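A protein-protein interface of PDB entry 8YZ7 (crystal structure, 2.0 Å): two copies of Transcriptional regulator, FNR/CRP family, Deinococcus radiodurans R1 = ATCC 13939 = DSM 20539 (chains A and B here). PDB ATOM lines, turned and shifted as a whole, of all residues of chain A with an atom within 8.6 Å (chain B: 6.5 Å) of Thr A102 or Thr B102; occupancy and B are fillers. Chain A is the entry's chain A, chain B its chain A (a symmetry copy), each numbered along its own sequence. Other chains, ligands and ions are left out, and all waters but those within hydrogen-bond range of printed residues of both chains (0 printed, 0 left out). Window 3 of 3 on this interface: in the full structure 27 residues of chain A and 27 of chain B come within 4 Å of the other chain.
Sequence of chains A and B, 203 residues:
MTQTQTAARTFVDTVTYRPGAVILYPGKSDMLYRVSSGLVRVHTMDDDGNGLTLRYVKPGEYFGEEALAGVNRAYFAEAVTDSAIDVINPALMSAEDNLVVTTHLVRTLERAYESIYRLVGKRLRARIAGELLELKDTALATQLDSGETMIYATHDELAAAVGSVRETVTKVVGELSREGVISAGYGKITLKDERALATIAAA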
ATOM      1  N   LEU A  32      -8.861  -6.934   0.325  1.00  0.00           N
ATOM      2  CA  LEU A  32      -8.281  -5.941   1.217  1.00  0.00           C
ATOM      3  C   LEU A  32      -9.242  -5.684   2.370  1.00  0.00           C
ATOM      4  O   LEU A  32     -10.461  -5.652   2.178  1.00  0.00           O
ATOM      5  CB  LEU A  32      -7.988  -4.632   0.478  1.00  0.00           C
ATOM      6  CG  LEU A  32      -7.382  -3.497   1.321  1.00  0.00           C
ATOM      7  CD1 LEU A  32      -5.948  -3.821   1.732  1.00  0.00           C
ATOM      8  CD2 LEU A  32      -7.451  -2.178   0.571  1.00  0.00           C
ATOM      9  N   TYR A  62      -5.619  -0.296   7.489  1.00  0.00           N
ATOM     10  CA  TYR A  62      -5.833  -1.416   6.586  1.00  0.00           C
ATOM     11  C   TYR A  62      -4.940  -2.596   6.962  1.00  0.00           C
ATOM     12  O   TYR A  62      -3.895  -2.433   7.594  1.00  0.00           O
ATOM     13  CB  TYR A  62      -5.556  -0.994   5.139  1.00  0.00           C
ATOM     14  CG  TYR A  62      -6.461   0.111   4.621  1.00  0.00           C
ATOM     15  CD1 TYR A  62      -6.238   1.444   4.962  1.00  0.00           C
ATOM     16  CD2 TYR A  62      -7.530  -0.178   3.780  1.00  0.00           C
ATOM     17  CE1 TYR A  62      -7.062   2.454   4.489  1.00  0.00           C
ATOM     18  CE2 TYR A  62      -8.359   0.829   3.300  1.00  0.00           C
ATOM     19  CZ  TYR A  62      -8.118   2.140   3.657  1.00  0.00           C
ATOM     20  OH  TYR A  62      -8.934   3.141   3.189  1.00  0.00           O
ATOM     21  N   GLU A  65      -2.958  -6.209   2.845  1.00  0.00           N
ATOM     22  CA  GLU A  65      -2.595  -5.445   1.618  1.00  0.00           C
ATOM     23  C   GLU A  65      -1.887  -6.317   0.577  1.00  0.00           C
ATOM     24  O   GLU A  65      -1.832  -5.894  -0.588  1.00  0.00           O
ATOM     25  CB  GLU A  65      -1.688  -4.267   1.965  1.00  0.00           C
ATOM     26  CG  GLU A  65      -2.224  -3.396   3.077  1.00  0.00           C
ATOM     27  CD  GLU A  65      -1.764  -3.841   4.452  1.00  0.00           C
ATOM     28  OE1 GLU A  65      -1.143  -4.918   4.552  1.00  0.00           O
ATOM     29  OE2 GLU A  65      -2.043  -3.119   5.426  1.00  0.00           O
ATOM     30  N   GLU A  66      -1.350  -7.469   0.973  1.00  0.00           N
ATOM     31  CA  GLU A  66      -0.725  -8.340  -0.015  1.00  0.00           C
ATOM     32  C   GLU A  66      -1.637  -8.594  -1.203  1.00  0.00           C
ATOM     33  O   GLU A  66      -1.149  -8.979  -2.271  1.00  0.00           O
ATOM     34  CB  GLU A  66      -0.334  -9.674   0.619  1.00  0.00           C
ATOM     35  CG  GLU A  66      -1.433 -10.293   1.457  1.00  0.00           C
ATOM     36  CD  GLU A  66      -1.433  -9.781   2.887  1.00  0.00           C
ATOM     37  OE1 GLU A  66      -0.550  -8.970   3.236  1.00  0.00           O
ATOM     38  OE2 GLU A  66      -2.310 -10.206   3.661  1.00  0.00           O
ATOM     39  N   ALA A  67      -2.945  -8.392  -1.039  1.00  0.00           N
ATOM     40  CA  ALA A  67      -3.871  -8.562  -2.152  1.00  0.00           C
ATOM     41  C   ALA A  67      -3.567  -7.586  -3.281  1.00  0.00           C
ATOM     42  O   ALA A  67      -3.750  -7.911  -4.460  1.00  0.00           O
ATOM     43  CB  ALA A  67      -5.308  -8.383  -1.667  1.00  0.00           C
ATOM     44  N   LEU A  68      -3.098  -6.382  -2.943  1.00  0.00           N
ATOM     45  CA  LEU A  68      -2.805  -5.393  -3.976  1.00  0.00           C
ATOM     46  C   LEU A  68      -1.710  -5.887  -4.913  1.00  0.00           C
ATOM     47  O   LEU A  68      -1.770  -5.662  -6.128  1.00  0.00           O
ATOM     48  CB  LEU A  68      -2.404  -4.070  -3.329  1.00  0.00           C
ATOM     49  CG  LEU A  68      -3.401  -3.568  -2.289  1.00  0.00           C
ATOM     50  CD1 LEU A  68      -2.892  -2.294  -1.656  1.00  0.00           C
ATOM     51  CD2 LEU A  68      -4.762  -3.357  -2.932  1.00  0.00           C
ATOM     52  N   ALA A  69      -0.714  -6.583  -4.367  1.00  0.00           N
ATOM     53  CA  ALA A  69       0.419  -7.099  -5.118  1.00  0.00           C
ATOM     54  C   ALA A  69       0.251  -8.561  -5.525  1.00  0.00           C
ATOM     55  O   ALA A  69       1.146  -9.117  -6.170  1.00  0.00           O
ATOM     56  CB  ALA A  69       1.702  -6.942  -4.296  1.00  0.00           C
ATOM     57  N   VAL A  71       0.757 -11.029  -3.907  1.00  0.00           N
ATOM     58  CA  VAL A  71       1.641 -11.876  -3.123  1.00  0.00           C
ATOM     59  C   VAL A  71       0.835 -12.613  -2.058  1.00  0.00           C
ATOM     60  O   VAL A  71      -0.248 -12.191  -1.645  1.00  0.00           O
ATOM     61  CB  VAL A  71       2.766 -11.033  -2.495  1.00  0.00           C
ATOM     62  CG1 VAL A  71       3.849 -11.903  -1.862  1.00  0.00           C
ATOM     63  CG2 VAL A  71       3.384 -10.127  -3.548  1.00  0.00           C
ATOM     64  N   MET A  93     -11.583  -0.841  -6.526  1.00  0.00           N
ATOM     65  CA  MET A  93     -11.181   0.423  -5.920  1.00  0.00           C
ATOM     66  C   MET A  93     -10.873   1.475  -6.978  1.00  0.00           C
ATOM     67  O   MET A  93     -10.364   1.178  -8.061  1.00  0.00           O
ATOM     68  CB  MET A  93      -9.956   0.234  -5.036  1.00  0.00           C
ATOM     69  CG  MET A  93     -10.231  -0.361  -3.689  1.00  0.00           C
ATOM     70  SD  MET A  93      -8.734  -0.165  -2.721  1.00  0.00           S
ATOM     71  CE  MET A  93      -7.531  -0.846  -3.860  1.00  0.00           C
ATOM     72  N   ALA A  95      -8.968   5.220  -8.089  1.00  0.00           N
ATOM     73  CA  ALA A  95      -7.632   5.781  -7.922  1.00  0.00           C
ATOM     74  C   ALA A  95      -7.529   6.616  -6.649  1.00  0.00           C
ATOM     75  O   ALA A  95      -6.490   6.617  -5.977  1.00  0.00           O
ATOM     76  CB  ALA A  95      -7.261   6.619  -9.142  1.00  0.00           C
ATOM     77  N   GLU A  96      -8.599   7.330  -6.298  1.00  0.00           N
ATOM     78  CA  GLU A  96      -8.588   8.115  -5.067  1.00  0.00           C
ATOM     79  C   GLU A  96      -8.393   7.220  -3.847  1.00  0.00           C
ATOM     80  O   GLU A  96      -7.591   7.529  -2.956  1.00  0.00           O
ATOM     81  CB  GLU A  96      -9.881   8.921  -4.952  1.00  0.00           C
ATOM     82  CG  GLU A  96     -10.043  10.014  -6.010  1.00  0.00           C
ATOM     83  CD  GLU A  96     -10.433   9.487  -7.386  1.00  0.00           C
ATOM     84  OE1 GLU A  96     -10.656   8.268  -7.528  1.00  0.00           O
ATOM     85  OE2 GLU A  96     -10.511  10.296  -8.332  1.00  0.00           O
ATOM     86  N   ASP A  97      -9.114   6.096  -3.797  1.00  0.00           N
ATOM     87  CA  ASP A  97      -8.953   5.152  -2.695  1.00  0.00           C
ATOM     88  C   ASP A  97      -7.549   4.563  -2.678  1.00  0.00           C
ATOM     89  O   ASP A  97      -6.983   4.312  -1.606  1.00  0.00           O
ATOM     90  CB  ASP A  97      -9.989   4.035  -2.809  1.00  0.00           C
ATOM     91  CG  ASP A  97     -11.404   4.564  -2.914  1.00  0.00           C
ATOM     92  OD1 ASP A  97     -11.800   5.368  -2.045  1.00  0.00           O
ATOM     93  OD2 ASP A  97     -12.113   4.191  -3.874  1.00  0.00           O
ATOM     94  N   ASN A  98      -6.976   4.330  -3.862  1.00  0.00           N
ATOM     95  CA  ASN A  98      -5.620   3.794  -3.948  1.00  0.00           C
ATOM     96  C   ASN A  98      -4.615   4.732  -3.299  1.00  0.00           C
ATOM     97  O   ASN A  98      -3.651   4.280  -2.671  1.00  0.00           O
ATOM     98  CB  ASN A  98      -5.247   3.546  -5.408  1.00  0.00           C
ATOM     99  CG  ASN A  98      -6.180   2.557  -6.083  1.00  0.00           C
ATOM    100  OD1 ASN A  98      -7.068   1.998  -5.440  1.00  0.00           O
ATOM    101  ND2 ASN A  98      -5.993   2.345  -7.383  1.00  0.00           N
ATOM    102  N   LEU A  99      -4.811   6.040  -3.455  1.00  0.00           N
ATOM    103  CA  LEU A  99      -3.916   6.995  -2.816  1.00  0.00           C
ATOM    104  C   LEU A  99      -4.022   6.924  -1.299  1.00  0.00           C
ATOM    105  O   LEU A  99      -3.028   7.112  -0.585  1.00  0.00           O
ATOM    106  CB  LEU A  99      -4.227   8.404  -3.301  1.00  0.00           C
ATOM    107  CG  LEU A  99      -3.436   9.516  -2.619  1.00  0.00           C
ATOM    108  CD1 LEU A  99      -1.999   9.521  -3.113  1.00  0.00           C
ATOM    109  CD2 LEU A  99      -4.106  10.859  -2.859  1.00  0.00           C
ATOM    110  N   VAL A 100      -5.230   6.670  -0.790  1.00  0.00           N
ATOM    111  CA  VAL A 100      -5.429   6.547   0.652  1.00  0.00           C
ATOM    112  C   VAL A 100      -4.669   5.346   1.187  1.00  0.00           C
ATOM    113  O   VAL A 100      -3.980   5.427   2.209  1.00  0.00           O
ATOM    114  CB  VAL A 100      -6.928   6.441   0.979  1.00  0.00           C
ATOM    115  CG1 VAL A 100      -7.131   6.223   2.471  1.00  0.00           C
ATOM    116  CG2 VAL A 100      -7.658   7.677   0.507  1.00  0.00           C
ATOM    117  N   VAL A 101      -4.808   4.206   0.515  1.00  0.00           N
ATOM    118  CA  VAL A 101      -4.130   2.997   0.965  1.00  0.00           C
ATOM    119  C   VAL A 101      -2.620   3.178   0.884  1.00  0.00           C
ATOM    120  O   VAL A 101      -1.881   2.724   1.763  1.00  0.00           O
ATOM    121  CB  VAL A 101      -4.611   1.786   0.145  1.00  0.00           C
ATOM    122  CG1 VAL A 101      -4.021   0.502   0.682  1.00  0.00           C
ATOM    123  CG2 VAL A 101      -6.125   1.713   0.161  1.00  0.00           C
ATOM    124  N   THR A 102      -2.140   3.859  -0.161  1.00  0.00           N
ATOM    125  CA  THR A 102      -0.707   4.086  -0.305  1.00  0.00           C
ATOM    126  C   THR A 102      -0.169   4.912   0.848  1.00  0.00           C
ATOM    127  O   THR A 102       0.907   4.620   1.383  1.00  0.00           O
ATOM    128  CB  THR A 102      -0.407   4.787  -1.626  1.00  0.00           C
ATOM    129  OG1 THR A 102      -0.881   3.989  -2.714  1.00  0.00           O
ATOM    130  CG2 THR A 102       1.088   5.006  -1.790  1.00  0.00           C
ATOM    131  N   THR A 103      -0.905   5.954   1.237  1.00  0.00           N
ATOM    132  CA  THR A 103      -0.498   6.764   2.377  1.00  0.00           C
ATOM    133  C   THR A 103      -0.425   5.927   3.645  1.00  0.00           C
ATOM    134  O   THR A 103       0.522   6.055   4.432  1.00  0.00           O
ATOM    135  CB  THR A 103      -1.478   7.925   2.555  1.00  0.00           C
ATOM    136  OG1 THR A 103      -1.437   8.754   1.395  1.00  0.00           O
ATOM    137  CG2 THR A 103      -1.134   8.756   3.781  1.00  0.00           C
ATOM    138  N   HIS A 104      -1.421   5.062   3.860  1.00  0.00           N
ATOM    139  CA  HIS A 104      -1.410   4.181   5.025  1.00  0.00           C
ATOM    140  C   HIS A 104      -0.221   3.226   4.988  1.00  0.00           C
ATOM    141  O   HIS A 104       0.417   2.979   6.022  1.00  0.00           O
ATOM    142  CB  HIS A 104      -2.724   3.402   5.102  1.00  0.00           C
ATOM    143  CG  HIS A 104      -2.640   2.159   5.940  1.00  0.00           C
ATOM    144  ND1 HIS A 104      -2.438   0.907   5.396  1.00  0.00           N
ATOM    145  CD2 HIS A 104      -2.719   1.976   7.282  1.00  0.00           C
ATOM    146  CE1 HIS A 104      -2.395   0.008   6.365  1.00  0.00           C
ATOM    147  NE2 HIS A 104      -2.566   0.631   7.519  1.00  0.00           N
ATOM    148  N   LEU A 105       0.089   2.674   3.813  1.00  0.00           N
ATOM    149  CA  LEU A 105       1.232   1.769   3.712  1.00  0.00           C
ATOM    150  C   LEU A 105       2.528   2.467   4.097  1.00  0.00           C
ATOM    151  O   LEU A 105       3.365   1.887   4.797  1.00  0.00           O
ATOM    152  CB  LEU A 105       1.348   1.193   2.300  1.00  0.00           C
ATOM    153  CG  LEU A 105       0.231   0.246   1.874  1.00  0.00           C
ATOM    154  CD1 LEU A 105       0.550  -0.388   0.534  1.00  0.00           C
ATOM    155  CD2 LEU A 105      -0.024  -0.819   2.936  1.00  0.00           C
ATOM    156  N   VAL A 106       2.721   3.704   3.639  1.00  0.00           N
ATOM    157  CA  VAL A 106       3.934   4.432   3.989  1.00  0.00           C
ATOM    158  C   VAL A 106       4.041   4.567   5.503  1.00  0.00           C
ATOM    159  O   VAL A 106       5.088   4.292   6.100  1.00  0.00           O
ATOM    160  CB  VAL A 106       3.965   5.802   3.281  1.00  0.00           C
ATOM    161  CG1 VAL A 106       5.101   6.658   3.798  1.00  0.00           C
ATOM    162  CG2 VAL A 106       4.113   5.623   1.769  1.00  0.00           C
ATOM    163  N   ARG A 107       2.948   4.955   6.157  1.00  0.00           N
ATOM    164  CA  ARG A 107       2.977   5.068   7.612  1.00  0.00           C
ATOM    165  C   ARG A 107       3.217   3.719   8.261  1.00  0.00           C
ATOM    166  O   ARG A 107       3.920   3.624   9.273  1.00  0.00           O
ATOM    167  CB  ARG A 107       1.675   5.655   8.130  1.00  0.00           C
ATOM    168  CG  ARG A 107       1.386   6.996   7.536  1.00  0.00           C
ATOM    169  CD  ARG A 107       0.007   7.439   7.937  1.00  0.00           C
ATOM    170  NE  ARG A 107      -0.350   8.680   7.267  1.00  0.00           N
ATOM    171  CZ  ARG A 107       0.100   9.877   7.618  1.00  0.00           C
ATOM    172  NH1 ARG A 107       0.922  10.033   8.647  1.00  0.00           N
ATOM    173  NH2 ARG A 107      -0.290  10.944   6.925  1.00  0.00           N
ATOM    174  N   THR A 108       2.618   2.666   7.709  1.00  0.00           N
ATOM    175  CA  THR A 108       2.800   1.351   8.307  1.00  0.00           C
ATOM    176  C   THR A 108       4.250   0.898   8.184  1.00  0.00           C
ATOM    177  O   THR A 108       4.809   0.319   9.123  1.00  0.00           O
ATOM    178  CB  THR A 108       1.852   0.341   7.662  1.00  0.00           C
ATOM    179  OG1 THR A 108       0.498   0.795   7.809  1.00  0.00           O
ATOM    180  CG2 THR A 108       1.978  -1.005   8.348  1.00  0.00           C
ATOM    181  N   LEU A 109       4.891   1.185   7.047  1.00  0.00           N
ATOM    182  CA  LEU A 109       6.303   0.839   6.902  1.00  0.00           C
ATOM    183  C   LEU A 109       7.164   1.658   7.853  1.00  0.00           C
ATOM    184  O   LEU A 109       8.152   1.153   8.403  1.00  0.00           O
ATOM    185  CB  LEU A 109       6.757   1.049   5.459  1.00  0.00           C
ATOM    186  CG  LEU A 109       8.223   0.712   5.182  1.00  0.00           C
ATOM    187  CD1 LEU A 109       8.458  -0.786   5.345  1.00  0.00           C
ATOM    188  CD2 LEU A 109       8.629   1.170   3.799  1.00  0.00           C
ATOM    189  N   LEU B  68       5.134  10.394  -0.709  1.00  0.00           N
ATOM    190  CA  LEU B  68       3.767  10.129  -1.145  1.00  0.00           C
ATOM    191  C   LEU B  68       2.760  10.563  -0.088  1.00  0.00           C
ATOM    192  O   LEU B  68       1.692  11.096  -0.414  1.00  0.00           O
ATOM    193  CB  LEU B  68       3.603   8.645  -1.467  1.00  0.00           C
ATOM    194  CG  LEU B  68       4.653   8.108  -2.436  1.00  0.00           C
ATOM    195  CD1 LEU B  68       4.455   6.624  -2.642  1.00  0.00           C
ATOM    196  CD2 LEU B  68       4.579   8.861  -3.753  1.00  0.00           C
ATOM    197  N   ALA B  69       3.095  10.363   1.186  1.00  0.00           N
ATOM    198  CA  ALA B  69       2.235  10.695   2.311  1.00  0.00           C
ATOM    199  C   ALA B  69       2.559  12.052   2.931  1.00  0.00           C
ATOM    200  O   ALA B  69       1.898  12.452   3.895  1.00  0.00           O
ATOM    201  CB  ALA B  69       2.338   9.606   3.382  1.00  0.00           C
ATOM    202  N   ASP B  97       1.768   4.227 -12.679  1.00  0.00           N
ATOM    203  CA  ASP B  97       2.994   4.238 -11.885  1.00  0.00           C
ATOM    204  C   ASP B  97       2.689   4.088 -10.401  1.00  0.00           C
ATOM    205  O   ASP B  97       3.447   3.447  -9.663  1.00  0.00           O
ATOM    206  CB  ASP B  97       3.764   5.533 -12.134  1.00  0.00           C
ATOM    207  CG  ASP B  97       4.026   5.779 -13.605  1.00  0.00           C
ATOM    208  OD1 ASP B  97       4.573   4.874 -14.267  1.00  0.00           O
ATOM    209  OD2 ASP B  97       3.669   6.870 -14.102  1.00  0.00           O
ATOM    210  N   ASN B  98       1.580   4.681  -9.948  1.00  0.00           N
ATOM    211  CA  ASN B  98       1.187   4.569  -8.547  1.00  0.00           C
ATOM    212  C   ASN B  98       0.941   3.120  -8.156  1.00  0.00           C
ATOM    213  O   ASN B  98       1.257   2.711  -7.035  1.00  0.00           O
ATOM    214  CB  ASN B  98      -0.062   5.408  -8.285  1.00  0.00           C
ATOM    215  CG  ASN B  98       0.153   6.878  -8.590  1.00  0.00           C
ATOM    216  OD1 ASN B  98       1.262   7.288  -8.931  1.00  0.00           O
ATOM    217  ND2 ASN B  98      -0.906   7.677  -8.481  1.00  0.00           N
ATOM    218  N   LEU B  99       0.361   2.335  -9.063  1.00  0.00           N
ATOM    219  CA  LEU B  99       0.144   0.923  -8.775  1.00  0.00           C
ATOM    220  C   LEU B  99       1.464   0.178  -8.633  1.00  0.00           C
ATOM    221  O   LEU B  99       1.581  -0.756  -7.829  1.00  0.00           O
ATOM    222  CB  LEU B  99      -0.701   0.294  -9.872  1.00  0.00           C
ATOM    223  CG  LEU B  99      -0.906  -1.215  -9.750  1.00  0.00           C
ATOM    224  CD1 LEU B  99      -1.886  -1.526  -8.633  1.00  0.00           C
ATOM    225  CD2 LEU B  99      -1.381  -1.787 -11.076  1.00  0.00           C
ATOM    226  N   VAL B 100       2.466   0.570  -9.422  1.00  0.00           N
ATOM    227  CA  VAL B 100       3.783  -0.058  -9.337  1.00  0.00           C
ATOM    228  C   VAL B 100       4.407   0.212  -7.981  1.00  0.00           C
ATOM    229  O   VAL B 100       4.942  -0.692  -7.330  1.00  0.00           O
ATOM    230  CB  VAL B 100       4.691   0.446 -10.473  1.00  0.00           C
ATOM    231  CG1 VAL B 100       6.088  -0.140 -10.332  1.00  0.00           C
ATOM    232  CG2 VAL B 100       4.092   0.103 -11.817  1.00  0.00           C
ATOM    233  N   VAL B 101       4.371   1.470  -7.547  1.00  0.00           N
ATOM    234  CA  VAL B 101       4.961   1.825  -6.264  1.00  0.00           C
ATOM    235  C   VAL B 101       4.221   1.127  -5.131  1.00  0.00           C
ATOM    236  O   VAL B 101       4.834   0.670  -4.160  1.00  0.00           O
ATOM    237  CB  VAL B 101       4.969   3.355  -6.091  1.00  0.00           C
ATOM    238  CG1 VAL B 101       5.696   3.753  -4.827  1.00  0.00           C
ATOM    239  CG2 VAL B 101       5.613   4.013  -7.296  1.00  0.00           C
ATOM    240  N   THR B 102       2.894   1.015  -5.244  1.00  0.00           N
ATOM    241  CA  THR B 102       2.114   0.349  -4.207  1.00  0.00           C
ATOM    242  C   THR B 102       2.514  -1.109  -4.078  1.00  0.00           C
ATOM    243  O   THR B 102       2.645  -1.628  -2.963  1.00  0.00           O
ATOM    244  CB  THR B 102       0.623   0.450  -4.514  1.00  0.00           C
ATOM    245  OG1 THR B 102       0.239   1.824  -4.598  1.00  0.00           O
ATOM    246  CG2 THR B 102      -0.195  -0.225  -3.425  1.00  0.00           C
ATOM    247  N   THR B 103       2.705  -1.783  -5.212  1.00  0.00           N
ATOM    248  CA  THR B 103       3.153  -3.170  -5.183  1.00  0.00           C
ATOM    249  C   THR B 103       4.507  -3.292  -4.500  1.00  0.00           C
ATOM    250  O   THR B 103       4.726  -4.204  -3.693  1.00  0.00           O
ATOM    251  CB  THR B 103       3.219  -3.715  -6.610  1.00  0.00           C
ATOM    252  OG1 THR B 103       1.912  -3.692  -7.180  1.00  0.00           O
ATOM    253  CG2 THR B 103       3.755  -5.137  -6.634  1.00  0.00           C
ATOM    254  N   HIS B 104       5.431  -2.377  -4.814  1.00  0.00           N
ATOM    255  CA  HIS B 104       6.742  -2.387  -4.172  1.00  0.00           C
ATOM    256  C   HIS B 104       6.627  -2.153  -2.669  1.00  0.00           C
ATOM    257  O   HIS B 104       7.324  -2.804  -1.877  1.00  0.00           O
ATOM    258  CB  HIS B 104       7.644  -1.330  -4.812  1.00  0.00           C
ATOM    259  CG  HIS B 104       8.804  -0.924  -3.950  1.00  0.00           C
ATOM    260  ND1 HIS B 104       8.784   0.207  -3.159  1.00  0.00           N
ATOM    261  CD2 HIS B 104      10.013  -1.502  -3.746  1.00  0.00           C
ATOM    262  CE1 HIS B 104       9.927   0.306  -2.504  1.00  0.00           C
ATOM    263  NE2 HIS B 104      10.693  -0.716  -2.846  1.00  0.00           N
ATOM    264  N   LEU B 105       5.759  -1.226  -2.255  1.00  0.00           N
ATOM    265  CA  LEU B 105       5.588  -0.975  -0.826  1.00  0.00           C
ATOM    266  C   LEU B 105       5.107  -2.220  -0.097  1.00  0.00           C
ATOM    267  O   LEU B 105       5.585  -2.526   1.001  1.00  0.00           O
ATOM    268  CB  LEU B 105       4.613   0.179  -0.588  1.00  0.00           C
ATOM    269  CG  LEU B 105       5.090   1.556  -1.037  1.00  0.00           C
ATOM    270  CD1 LEU B 105       4.117   2.630  -0.590  1.00  0.00           C
ATOM    271  CD2 LEU B 105       6.497   1.846  -0.524  1.00  0.00           C
ATOM    272  N   VAL B 106       4.151  -2.946  -0.681  1.00  0.00           N
ATOM    273  CA  VAL B 106       3.662  -4.161  -0.041  1.00  0.00           C
ATOM    274  C   VAL B 106       4.812  -5.140   0.161  1.00  0.00           C
ATOM    275  O   VAL B 106       4.997  -5.696   1.251  1.00  0.00           O
ATOM    276  CB  VAL B 106       2.512  -4.778  -0.863  1.00  0.00           C
ATOM    277  CG1 VAL B 106       2.140  -6.147  -0.337  1.00  0.00           C
ATOM    278  CG2 VAL B 106       1.280  -3.871  -0.831  1.00  0.00           C
ATOM    279  N   ARG B 107       5.628  -5.342  -0.871  1.00  0.00           N
ATOM    280  CA  ARG B 107       6.768  -6.242  -0.727  1.00  0.00           C
ATOM    281  C   ARG B 107       7.753  -5.717   0.298  1.00  0.00           C
ATOM    282  O   ARG B 107       8.345  -6.493   1.056  1.00  0.00           O
ATOM    283  CB  ARG B 107       7.475  -6.428  -2.060  1.00  0.00           C
ATOM    284  CG  ARG B 107       6.558  -6.957  -3.114  1.00  0.00           C
ATOM    285  CD  ARG B 107       7.256  -6.943  -4.446  1.00  0.00           C
ATOM    286  NE  ARG B 107       6.344  -7.330  -5.510  1.00  0.00           N
ATOM    287  CZ  ARG B 107       5.969  -8.578  -5.759  1.00  0.00           C
ATOM    288  NH1 ARG B 107       6.425  -9.594  -5.040  1.00  0.00           N
ATOM    289  NH2 ARG B 107       5.121  -8.813  -6.757  1.00  0.00           N
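The side-chain hydroxyl of Thr B102 lies within hydrogen-bond range of the side-chain hydroxyl of Thr A102 (3.1 Å).
O of Glu A66 lies within hydrogen-bond range of N of Val A71. The backbone carbonyl oxygen (O) of Asn A98 lies within hydrogen-bond range of the side-chain hydroxyl (OG1) of Thr A102 (2.8 Å). The backbone carbonyl oxygen (O) of Leu A99 is in hydrogen-bond range of the side-chain hydroxyl (OG1) of Thr A103, at 3.0 Å. The backbone carbonyl oxygen (O) of Asn B98 is in hydrogen-bond range of the side-chain hydroxyl (OG1) of Thr B102 (2.8 Å). O of Leu B99 lies within hydrogen-bond range of OG1 of Thr B103 (3.0 Å).
Among the printed residues, pairs that only touch across the chains: Val A71 with Arg B107, Thr A103 with Ala B69, Ala A69 with Thr B103, Glu A66 with Val B106, Glu A65 with Val B106, Val A106 with Leu B105, Leu A105 with Val B106, Thr A102 with Leu B68 and Leu A68 with Thr B102.
Thr A102 touches two residues of chain B. Thr B102 touches just these residues of chain A: Leu A68 (3.8 Å) and Thr A102 (3.1 Å). Of the printed residues of chain A, Arg B107 touches Val A71 (3.4 Å). Printed residues of chain A within 4 Å of Thr B103: Ala A69. Of the printed residues of chain B, Thr A103 touches Ala B69. Of the printed residues of chain B, Val A71 touches Arg B107 (3.4 Å). Met A93 touches none of the printed residues of chain B. Tyr A62 touches none of the printed residues of chain B. The nearest residue of chain A that does not touch Thr B102 is Leu A105 (4.03 Å).
Of the 13 printed residues of chain B, 7 touch a printed residue of chain A. Of the 24 printed residues of chain A, 9 touch a printed residue of chain B. Among the printed residues, 10 pairs touch across the chains.
Leu A68 touches Thr B102, and with the chains exchanged Thr A102 touches Leu B68. Ala A69 touches Thr B103, and with the chains exchanged Thr A103 touches Ala B69. Thr A102 touches its own counterpart, Thr B102. Leu A105 touches Val B106, and with the chains exchanged Val A106 touches Leu B105. Of the 10 pairs that touch across the chains among the printed residues, 7 have their exchanged pair printed and touching as well.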
